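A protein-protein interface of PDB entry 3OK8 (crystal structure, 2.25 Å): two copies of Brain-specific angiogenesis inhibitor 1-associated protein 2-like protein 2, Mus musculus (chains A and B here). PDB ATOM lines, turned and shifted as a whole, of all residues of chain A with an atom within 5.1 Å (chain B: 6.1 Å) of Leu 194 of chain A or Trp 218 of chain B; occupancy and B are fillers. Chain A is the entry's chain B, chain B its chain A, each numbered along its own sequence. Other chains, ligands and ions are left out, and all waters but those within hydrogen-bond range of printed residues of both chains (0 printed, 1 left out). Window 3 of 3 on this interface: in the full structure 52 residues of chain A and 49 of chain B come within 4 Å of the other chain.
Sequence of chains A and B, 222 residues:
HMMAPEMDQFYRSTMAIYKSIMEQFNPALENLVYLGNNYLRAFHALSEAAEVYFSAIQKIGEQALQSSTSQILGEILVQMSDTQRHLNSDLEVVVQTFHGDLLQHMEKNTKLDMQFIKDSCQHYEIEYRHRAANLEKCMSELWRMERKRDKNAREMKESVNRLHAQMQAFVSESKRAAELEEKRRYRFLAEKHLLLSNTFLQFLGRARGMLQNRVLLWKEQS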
ATOM      1  N   ALA A 190       1.798  23.311 -30.792  1.00  0.00           N
ATOM      2  CA  ALA A 190       3.012  22.575 -30.465  1.00  0.00           C
ATOM      3  C   ALA A 190       4.282  23.196 -31.050  1.00  0.00           C
ATOM      4  O   ALA A 190       5.283  23.307 -30.345  1.00  0.00           O
ATOM      5  CB  ALA A 190       2.893  21.106 -30.872  1.00  0.00           C
ATOM      6  N   GLU A 191       4.251  23.597 -32.320  1.00  0.00           N
ATOM      7  CA  GLU A 191       5.412  24.241 -32.932  1.00  0.00           C
ATOM      8  C   GLU A 191       5.820  25.517 -32.179  1.00  0.00           C
ATOM      9  O   GLU A 191       7.004  25.762 -31.971  1.00  0.00           O
ATOM     10  CB  GLU A 191       5.156  24.590 -34.391  1.00  0.00           C
ATOM     11  CG  GLU A 191       5.118  23.386 -35.338  1.00  0.00           C
ATOM     12  CD  GLU A 191       4.961  23.809 -36.789  1.00  0.00           C
ATOM     13  OE1 GLU A 191       4.352  24.876 -37.042  1.00  0.00           O
ATOM     14  OE2 GLU A 191       5.457  23.082 -37.675  1.00  0.00           O
ATOM     15  N   LYS A 192       4.837  26.323 -31.788  1.00  0.00           N
ATOM     16  CA  LYS A 192       5.100  27.585 -31.102  1.00  0.00           C
ATOM     17  C   LYS A 192       5.754  27.367 -29.752  1.00  0.00           C
ATOM     18  O   LYS A 192       6.727  28.036 -29.424  1.00  0.00           O
ATOM     19  CB  LYS A 192       3.824  28.428 -30.948  1.00  0.00           C
ATOM     20  CG  LYS A 192       3.634  29.485 -32.033  1.00  0.00           C
ATOM     21  CD  LYS A 192       4.391  29.127 -33.305  1.00  0.00           C
ATOM     22  CE  LYS A 192       4.292  30.235 -34.360  1.00  0.00           C
ATOM     23  NZ  LYS A 192       4.972  31.506 -33.950  1.00  0.00           N
ATOM     24  N   HIS A 193       5.235  26.431 -28.968  1.00  0.00           N
ATOM     25  CA  HIS A 193       5.843  26.156 -27.670  1.00  0.00           C
ATOM     26  C   HIS A 193       7.179  25.402 -27.746  1.00  0.00           C
ATOM     27  O   HIS A 193       7.987  25.503 -26.826  1.00  0.00           O
ATOM     28  CB  HIS A 193       4.852  25.464 -26.730  1.00  0.00           C
ATOM     29  CG  HIS A 193       3.653  26.304 -26.402  1.00  0.00           C
ATOM     30  ND1 HIS A 193       2.705  26.638 -27.340  1.00  0.00           N
ATOM     31  CD2 HIS A 193       3.260  26.890 -25.247  1.00  0.00           C
ATOM     32  CE1 HIS A 193       1.773  27.387 -26.778  1.00  0.00           C
ATOM     33  NE2 HIS A 193       2.085  27.554 -25.506  1.00  0.00           N
ATOM     34  N   LEU A 194       7.426  24.672 -28.832  1.00  0.00           N
ATOM     35  CA  LEU A 194       8.751  24.071 -29.044  1.00  0.00           C
ATOM     36  C   LEU A 194       9.782  25.173 -29.287  1.00  0.00           C
ATOM     37  O   LEU A 194      10.931  25.080 -28.846  1.00  0.00           O
ATOM     38  CB  LEU A 194       8.734  23.143 -30.250  1.00  0.00           C
ATOM     39  CG  LEU A 194       9.631  21.904 -30.351  1.00  0.00           C
ATOM     40  CD1 LEU A 194       9.972  21.651 -31.810  1.00  0.00           C
ATOM     41  CD2 LEU A 194      10.895  22.007 -29.540  1.00  0.00           C
ATOM     42  N   LEU A 195       9.365  26.210 -30.008  1.00  0.00           N
ATOM     43  CA  LEU A 195      10.208  27.367 -30.288  1.00  0.00           C
ATOM     44  C   LEU A 195      10.491  28.130 -29.004  1.00  0.00           C
ATOM     45  O   LEU A 195      11.616  28.532 -28.748  1.00  0.00           O
ATOM     46  CB  LEU A 195       9.526  28.277 -31.315  1.00  0.00           C
ATOM     47  CG  LEU A 195       9.953  29.743 -31.429  1.00  0.00           C
ATOM     48  CD1 LEU A 195      11.367  29.857 -31.970  1.00  0.00           C
ATOM     49  CD2 LEU A 195       8.967  30.512 -32.307  1.00  0.00           C
ATOM     50  N   LEU A 196       9.461  28.323 -28.193  1.00  0.00           N
ATOM     51  CA  LEU A 196       9.630  28.967 -26.907  1.00  0.00           C
ATOM     52  C   LEU A 196      10.625  28.197 -26.031  1.00  0.00           C
ATOM     53  O   LEU A 196      11.459  28.790 -25.331  1.00  0.00           O
ATOM     54  CB  LEU A 196       8.287  29.051 -26.198  1.00  0.00           C
ATOM     55  CG  LEU A 196       8.373  29.659 -24.802  1.00  0.00           C
ATOM     56  CD1 LEU A 196       8.866  31.094 -24.921  1.00  0.00           C
ATOM     57  CD2 LEU A 196       7.021  29.586 -24.104  1.00  0.00           C
ATOM     58  N   SER A 197      10.525  26.872 -26.093  1.00  0.00           N
ATOM     59  CA  SER A 197      11.349  25.959 -25.320  1.00  0.00           C
ATOM     60  C   SER A 197      12.810  26.037 -25.717  1.00  0.00           C
ATOM     61  O   SER A 197      13.688  25.963 -24.860  1.00  0.00           O
ATOM     62  CB  SER A 197      10.865  24.519 -25.498  1.00  0.00           C
ATOM     63  OG  SER A 197       9.680  24.276 -24.758  1.00  0.00           O
ATOM     64  N   ASN A 198      13.066  26.158 -27.015  1.00  0.00           N
ATOM     65  CA  ASN A 198      14.429  26.285 -27.506  1.00  0.00           C
ATOM     66  C   ASN A 198      15.051  27.640 -27.188  1.00  0.00           C
ATOM     67  O   ASN A 198      16.237  27.732 -26.839  1.00  0.00           O
ATOM     68  CB  ASN A 198      14.476  26.025 -28.997  1.00  0.00           C
ATOM     69  CG  ASN A 198      14.487  24.558 -29.312  1.00  0.00           C
ATOM     70  OD1 ASN A 198      15.281  23.807 -28.743  1.00  0.00           O
ATOM     71  ND2 ASN A 198      13.603  24.127 -30.213  1.00  0.00           N
ATOM     72  N   GLU B  75       0.271  14.027 -27.401  1.00  0.00           N
ATOM     73  CA  GLU B  75       1.261  13.563 -26.435  1.00  0.00           C
ATOM     74  C   GLU B  75       2.259  14.666 -26.099  1.00  0.00           C
ATOM     75  O   GLU B  75       2.611  14.844 -24.950  1.00  0.00           O
ATOM     76  CB  GLU B  75       2.005  12.331 -26.949  1.00  0.00           C
ATOM     77  CG  GLU B  75       1.145  11.060 -27.069  1.00  0.00           C
ATOM     78  CD  GLU B  75       0.665  10.523 -25.720  1.00  0.00           C
ATOM     79  OE1 GLU B  75       0.037   9.439 -25.699  1.00  0.00           O
ATOM     80  OE2 GLU B  75       0.906  11.182 -24.682  1.00  0.00           O
ATOM     81  N   ILE B  76       2.694  15.404 -27.112  1.00  0.00           N
ATOM     82  CA  ILE B  76       3.666  16.459 -26.942  1.00  0.00           C
ATOM     83  C   ILE B  76       3.205  17.569 -26.003  1.00  0.00           C
ATOM     84  O   ILE B  76       3.974  18.020 -25.148  1.00  0.00           O
ATOM     85  CB  ILE B  76       4.080  17.043 -28.296  1.00  0.00           C
ATOM     86  CG1 ILE B  76       4.848  15.983 -29.091  1.00  0.00           C
ATOM     87  CG2 ILE B  76       4.890  18.323 -28.078  1.00  0.00           C
ATOM     88  CD1 ILE B  76       5.142  16.344 -30.534  1.00  0.00           C
ATOM     89  N   GLN B  79       3.058  16.498 -22.375  1.00  0.00           N
ATOM     90  CA  GLN B  79       4.374  16.420 -21.735  1.00  0.00           C
ATOM     91  C   GLN B  79       5.113  17.749 -21.672  1.00  0.00           C
ATOM     92  O   GLN B  79       6.179  17.847 -21.083  1.00  0.00           O
ATOM     93  CB  GLN B  79       5.258  15.309 -22.306  1.00  0.00           C
ATOM     94  CG  GLN B  79       5.289  15.156 -23.795  1.00  0.00           C
ATOM     95  CD  GLN B  79       6.063  13.909 -24.194  1.00  0.00           C
ATOM     96  OE1 GLN B  79       7.190  13.705 -23.740  1.00  0.00           O
ATOM     97  NE2 GLN B  79       5.460  13.065 -25.033  1.00  0.00           N
ATOM     98  N   MET B  80       4.535  18.778 -22.270  1.00  0.00           N
ATOM     99  CA  MET B  80       5.054  20.116 -22.090  1.00  0.00           C
ATOM    100  C   MET B  80       4.568  20.637 -20.756  1.00  0.00           C
ATOM    101  O   MET B  80       5.339  21.222 -19.993  1.00  0.00           O
ATOM    102  CB  MET B  80       4.608  21.036 -23.216  1.00  0.00           C
ATOM    103  CG  MET B  80       5.381  20.885 -24.506  1.00  0.00           C
ATOM    104  SD  MET B  80       4.622  21.858 -25.830  1.00  0.00           S
ATOM    105  CE  MET B  80       5.873  21.729 -27.102  1.00  0.00           C
ATOM    106  N   THR B  83       6.419  18.862 -18.045  1.00  0.00           N
ATOM    107  CA  THR B  83       7.759  19.444 -17.903  1.00  0.00           C
ATOM    108  C   THR B  83       7.744  20.726 -17.092  1.00  0.00           C
ATOM    109  O   THR B  83       8.573  20.915 -16.193  1.00  0.00           O
ATOM    110  CB  THR B  83       8.386  19.792 -19.259  1.00  0.00           C
ATOM    111  OG1 THR B  83       8.483  18.610 -20.054  1.00  0.00           O
ATOM    112  CG2 THR B  83       9.796  20.393 -19.073  1.00  0.00           C
ATOM    113  N   LEU B 211      15.635  20.031 -20.862  1.00  0.00           N
ATOM    114  CA  LEU B 211      15.223  20.740 -22.060  1.00  0.00           C
ATOM    115  C   LEU B 211      16.076  20.380 -23.265  1.00  0.00           C
ATOM    116  O   LEU B 211      15.648  20.561 -24.400  1.00  0.00           O
ATOM    117  CB  LEU B 211      15.201  22.253 -21.843  1.00  0.00           C
ATOM    118  CG  LEU B 211      13.998  22.759 -21.047  1.00  0.00           C
ATOM    119  CD1 LEU B 211      13.878  24.262 -21.166  1.00  0.00           C
ATOM    120  CD2 LEU B 211      12.715  22.098 -21.535  1.00  0.00           C
ATOM    121  N   ASN B 213      16.898  17.438 -24.096  1.00  0.00           N
ATOM    122  CA  ASN B 213      16.277  16.269 -24.678  1.00  0.00           C
ATOM    123  C   ASN B 213      14.828  16.542 -25.081  1.00  0.00           C
ATOM    124  O   ASN B 213      14.441  16.172 -26.176  1.00  0.00           O
ATOM    125  CB  ASN B 213      16.412  15.046 -23.764  1.00  0.00           C
ATOM    126  CG  ASN B 213      15.406  15.043 -22.639  1.00  0.00           C
ATOM    127  OD1 ASN B 213      14.223  14.755 -22.844  1.00  0.00           O
ATOM    128  ND2 ASN B 213      15.868  15.366 -21.439  1.00  0.00           N
ATOM    129  N   ARG B 214      14.036  17.206 -24.235  1.00  0.00           N
ATOM    130  CA  ARG B 214      12.660  17.494 -24.606  1.00  0.00           C
ATOM    131  C   ARG B 214      12.604  18.127 -25.987  1.00  0.00           C
ATOM    132  O   ARG B 214      11.860  17.674 -26.839  1.00  0.00           O
ATOM    133  CB  ARG B 214      11.978  18.414 -23.589  1.00  0.00           C
ATOM    134  CG  ARG B 214      11.770  17.826 -22.201  1.00  0.00           C
ATOM    135  CD  ARG B 214      11.191  16.435 -22.225  1.00  0.00           C
ATOM    136  NE  ARG B 214      10.855  15.984 -20.876  1.00  0.00           N
ATOM    137  CZ  ARG B 214      11.751  15.648 -19.950  1.00  0.00           C
ATOM    138  NH1 ARG B 214      11.350  15.249 -18.751  1.00  0.00           N
ATOM    139  NH2 ARG B 214      13.051  15.710 -20.218  1.00  0.00           N
ATOM    140  N   VAL B 215      13.390  19.175 -26.204  1.00  0.00           N
ATOM    141  CA  VAL B 215      13.395  19.852 -27.503  1.00  0.00           C
ATOM    142  C   VAL B 215      13.644  18.888 -28.681  1.00  0.00           C
ATOM    143  O   VAL B 215      13.178  19.114 -29.800  1.00  0.00           O
ATOM    144  CB  VAL B 215      14.385  21.047 -27.545  1.00  0.00           C
ATOM    145  CG1 VAL B 215      14.060  22.054 -26.417  1.00  0.00           C
ATOM    146  CG2 VAL B 215      15.839  20.570 -27.448  1.00  0.00           C
ATOM    147  N   LEU B 216      14.376  17.816 -28.416  1.00  0.00           N
ATOM    148  CA  LEU B 216      14.642  16.799 -29.428  1.00  0.00           C
ATOM    149  C   LEU B 216      13.466  15.831 -29.582  1.00  0.00           C
ATOM    150  O   LEU B 216      13.080  15.478 -30.702  1.00  0.00           O
ATOM    151  CB  LEU B 216      15.921  16.031 -29.083  1.00  0.00           C
ATOM    152  CG  LEU B 216      17.223  16.821 -29.211  1.00  0.00           C
ATOM    153  CD1 LEU B 216      18.367  16.098 -28.506  1.00  0.00           C
ATOM    154  CD2 LEU B 216      17.550  17.078 -30.682  1.00  0.00           C
ATOM    155  N   LEU B 217      12.886  15.407 -28.463  1.00  0.00           N
ATOM    156  CA  LEU B 217      11.771  14.465 -28.531  1.00  0.00           C
ATOM    157  C   LEU B 217      10.498  15.111 -29.104  1.00  0.00           C
ATOM    158  O   LEU B 217       9.621  14.427 -29.639  1.00  0.00           O
ATOM    159  CB  LEU B 217      11.496  13.860 -27.156  1.00  0.00           C
ATOM    160  CG  LEU B 217      12.673  13.121 -26.507  1.00  0.00           C
ATOM    161  CD1 LEU B 217      12.345  12.672 -25.087  1.00  0.00           C
ATOM    162  CD2 LEU B 217      13.111  11.947 -27.359  1.00  0.00           C
ATOM    163  N   TRP B 218      10.418  16.432 -29.007  1.00  0.00           N
ATOM    164  CA  TRP B 218       9.231  17.162 -29.437  1.00  0.00           C
ATOM    165  C   TRP B 218       9.337  17.709 -30.855  1.00  0.00           C
ATOM    166  O   TRP B 218       8.492  18.486 -31.282  1.00  0.00           O
ATOM    167  CB  TRP B 218       8.935  18.323 -28.485  1.00  0.00           C
ATOM    168  CG  TRP B 218       8.619  17.927 -27.075  1.00  0.00           C
ATOM    169  CD1 TRP B 218       8.139  16.717 -26.637  1.00  0.00           C
ATOM    170  CD2 TRP B 218       8.713  18.765 -25.921  1.00  0.00           C
ATOM    171  NE1 TRP B 218       7.952  16.755 -25.267  1.00  0.00           N
ATOM    172  CE2 TRP B 218       8.297  17.999 -24.808  1.00  0.00           C
ATOM    173  CE3 TRP B 218       9.128  20.088 -25.713  1.00  0.00           C
ATOM    174  CZ2 TRP B 218       8.280  18.517 -23.508  1.00  0.00           C
ATOM    175  CZ3 TRP B 218       9.112  20.601 -24.420  1.00  0.00           C
ATOM    176  CH2 TRP B 218       8.692  19.814 -23.335  1.00  0.00           C
ATOM    177  N   LYS B 219      10.377  17.338 -31.544  1.00  0.00           N
ATOM    178  CA  LYS B 219      10.498  17.732 -32.888  1.00  0.00           C
ATOM    179  C   LYS B 219       9.548  16.746 -33.523  1.00  0.00           C
ATOM    180  O   LYS B 219       9.249  15.713 -32.968  1.00  0.00           O
ATOM    181  CB  LYS B 219      11.894  17.486 -33.402  1.00  0.00           C
ATOM    182  CG  LYS B 219      12.823  18.662 -33.425  1.00  0.00           C
ATOM    183  CD  LYS B 219      14.000  18.408 -34.328  1.00  0.00           C
ATOM    184  CE  LYS B 219      15.026  17.449 -33.713  1.00  0.00           C
ATOM    185  NZ  LYS B 219      14.480  16.160 -33.212  1.00  0.00           N
ATOM    186  N   GLU B 220       9.030  17.066 -34.677  1.00  0.00           N
ATOM    187  CA  GLU B 220       8.180  16.077 -35.264  1.00  0.00           C
ATOM    188  C   GLU B 220       8.725  15.500 -36.520  1.00  0.00           C
ATOM    189  O   GLU B 220       8.081  14.691 -37.125  1.00  0.00           O
ATOM    190  CB  GLU B 220       6.720  16.493 -35.328  1.00  0.00           C
ATOM    191  CG  GLU B 220       5.990  15.820 -34.226  1.00  0.00           C
ATOM    192  CD  GLU B 220       6.663  14.520 -33.914  1.00  0.00           C
ATOM    193  OE1 GLU B 220       7.117  13.905 -34.875  1.00  0.00           O
ATOM    194  OE2 GLU B 220       6.743  14.116 -32.737  1.00  0.00           O
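Among the printed residues, merely in contact across the chains: Ala 190 of chain A with Met 80 of chain B (3.7 Å), His 193 of chain A with Met 80 of chain B (3.7 Å), Leu 194 of chain A with Met 80 of chain B (3.8 Å), Leu 194 of chain A with Val 215 of chain B (3.7 Å), Leu 194 of chain A with Trp 218 of chain B (3.5 Å), Ser 197 of chain A with Trp 218 of chain B (3.7 Å) and Asn 198 of chain A with Val 215 of chain B (3.1 Å).
Printed residues of chain A that touch a printed residue of chain B: Ala 190, His 193, Leu 194, Ser 197 and Asn 198.
Printed residues of chain B that touch a printed residue of chain A: Met 80, Val 215 and Trp 218.
Hydrophobic or aromatic side chains of chain B that line the printed part of chain A: Met 80, Val 215 and Trp 218.
The side-chain amide oxygen (OE1) of Gln 79 of chain B sits close to the indole nitrogen (NE1) of Trp 218 of chain B (3.5 Å).
O of His 193 of chain A is in hydrogen-bond range of OG of Ser 197 of chain A (2.9 Å).
ND2 of Asn 198 of chain A lies within hydrogen-bond range of O of Leu 194 of chain A (3.1 Å).
Leu 194 of chain A touches just these residues of chain B: Met 80, Val 215 and Trp 218.
Trp 218 of chain B touches just these residues of chain A: Leu 194 and Ser 197.
Printed residues of chain A within 4 Å of Val 215 of chain B: Leu 194 and Asn 198.
Of the printed residues of chain B, Ala 190 of chain A touches Met 80.
Of the printed residues of chain B, Asn 198 of chain A touches Val 215 (3.1 Å).
Of the printed residues of chain A, Met 80 of chain B touches Ala 190 (3.7 Å), His 193 (3.7 Å) and Leu 194 (3.8 Å).
Of the printed residues of chain B, His 193 of chain A touches Met 80 (3.7 Å).
Leu 216 of chain B touches none of the printed residues of chain A.
Lys 219 of chain B touches none of the printed residues of chain A.
The nearest printed residue of chain A that does not touch Trp 218 of chain B is His 193 of chain A (5.6 Å).
No position is printed for both chains.
Of the 7 pairs that touch across the chains among the printed residues, none has its exchanged pair printed and touching as well.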
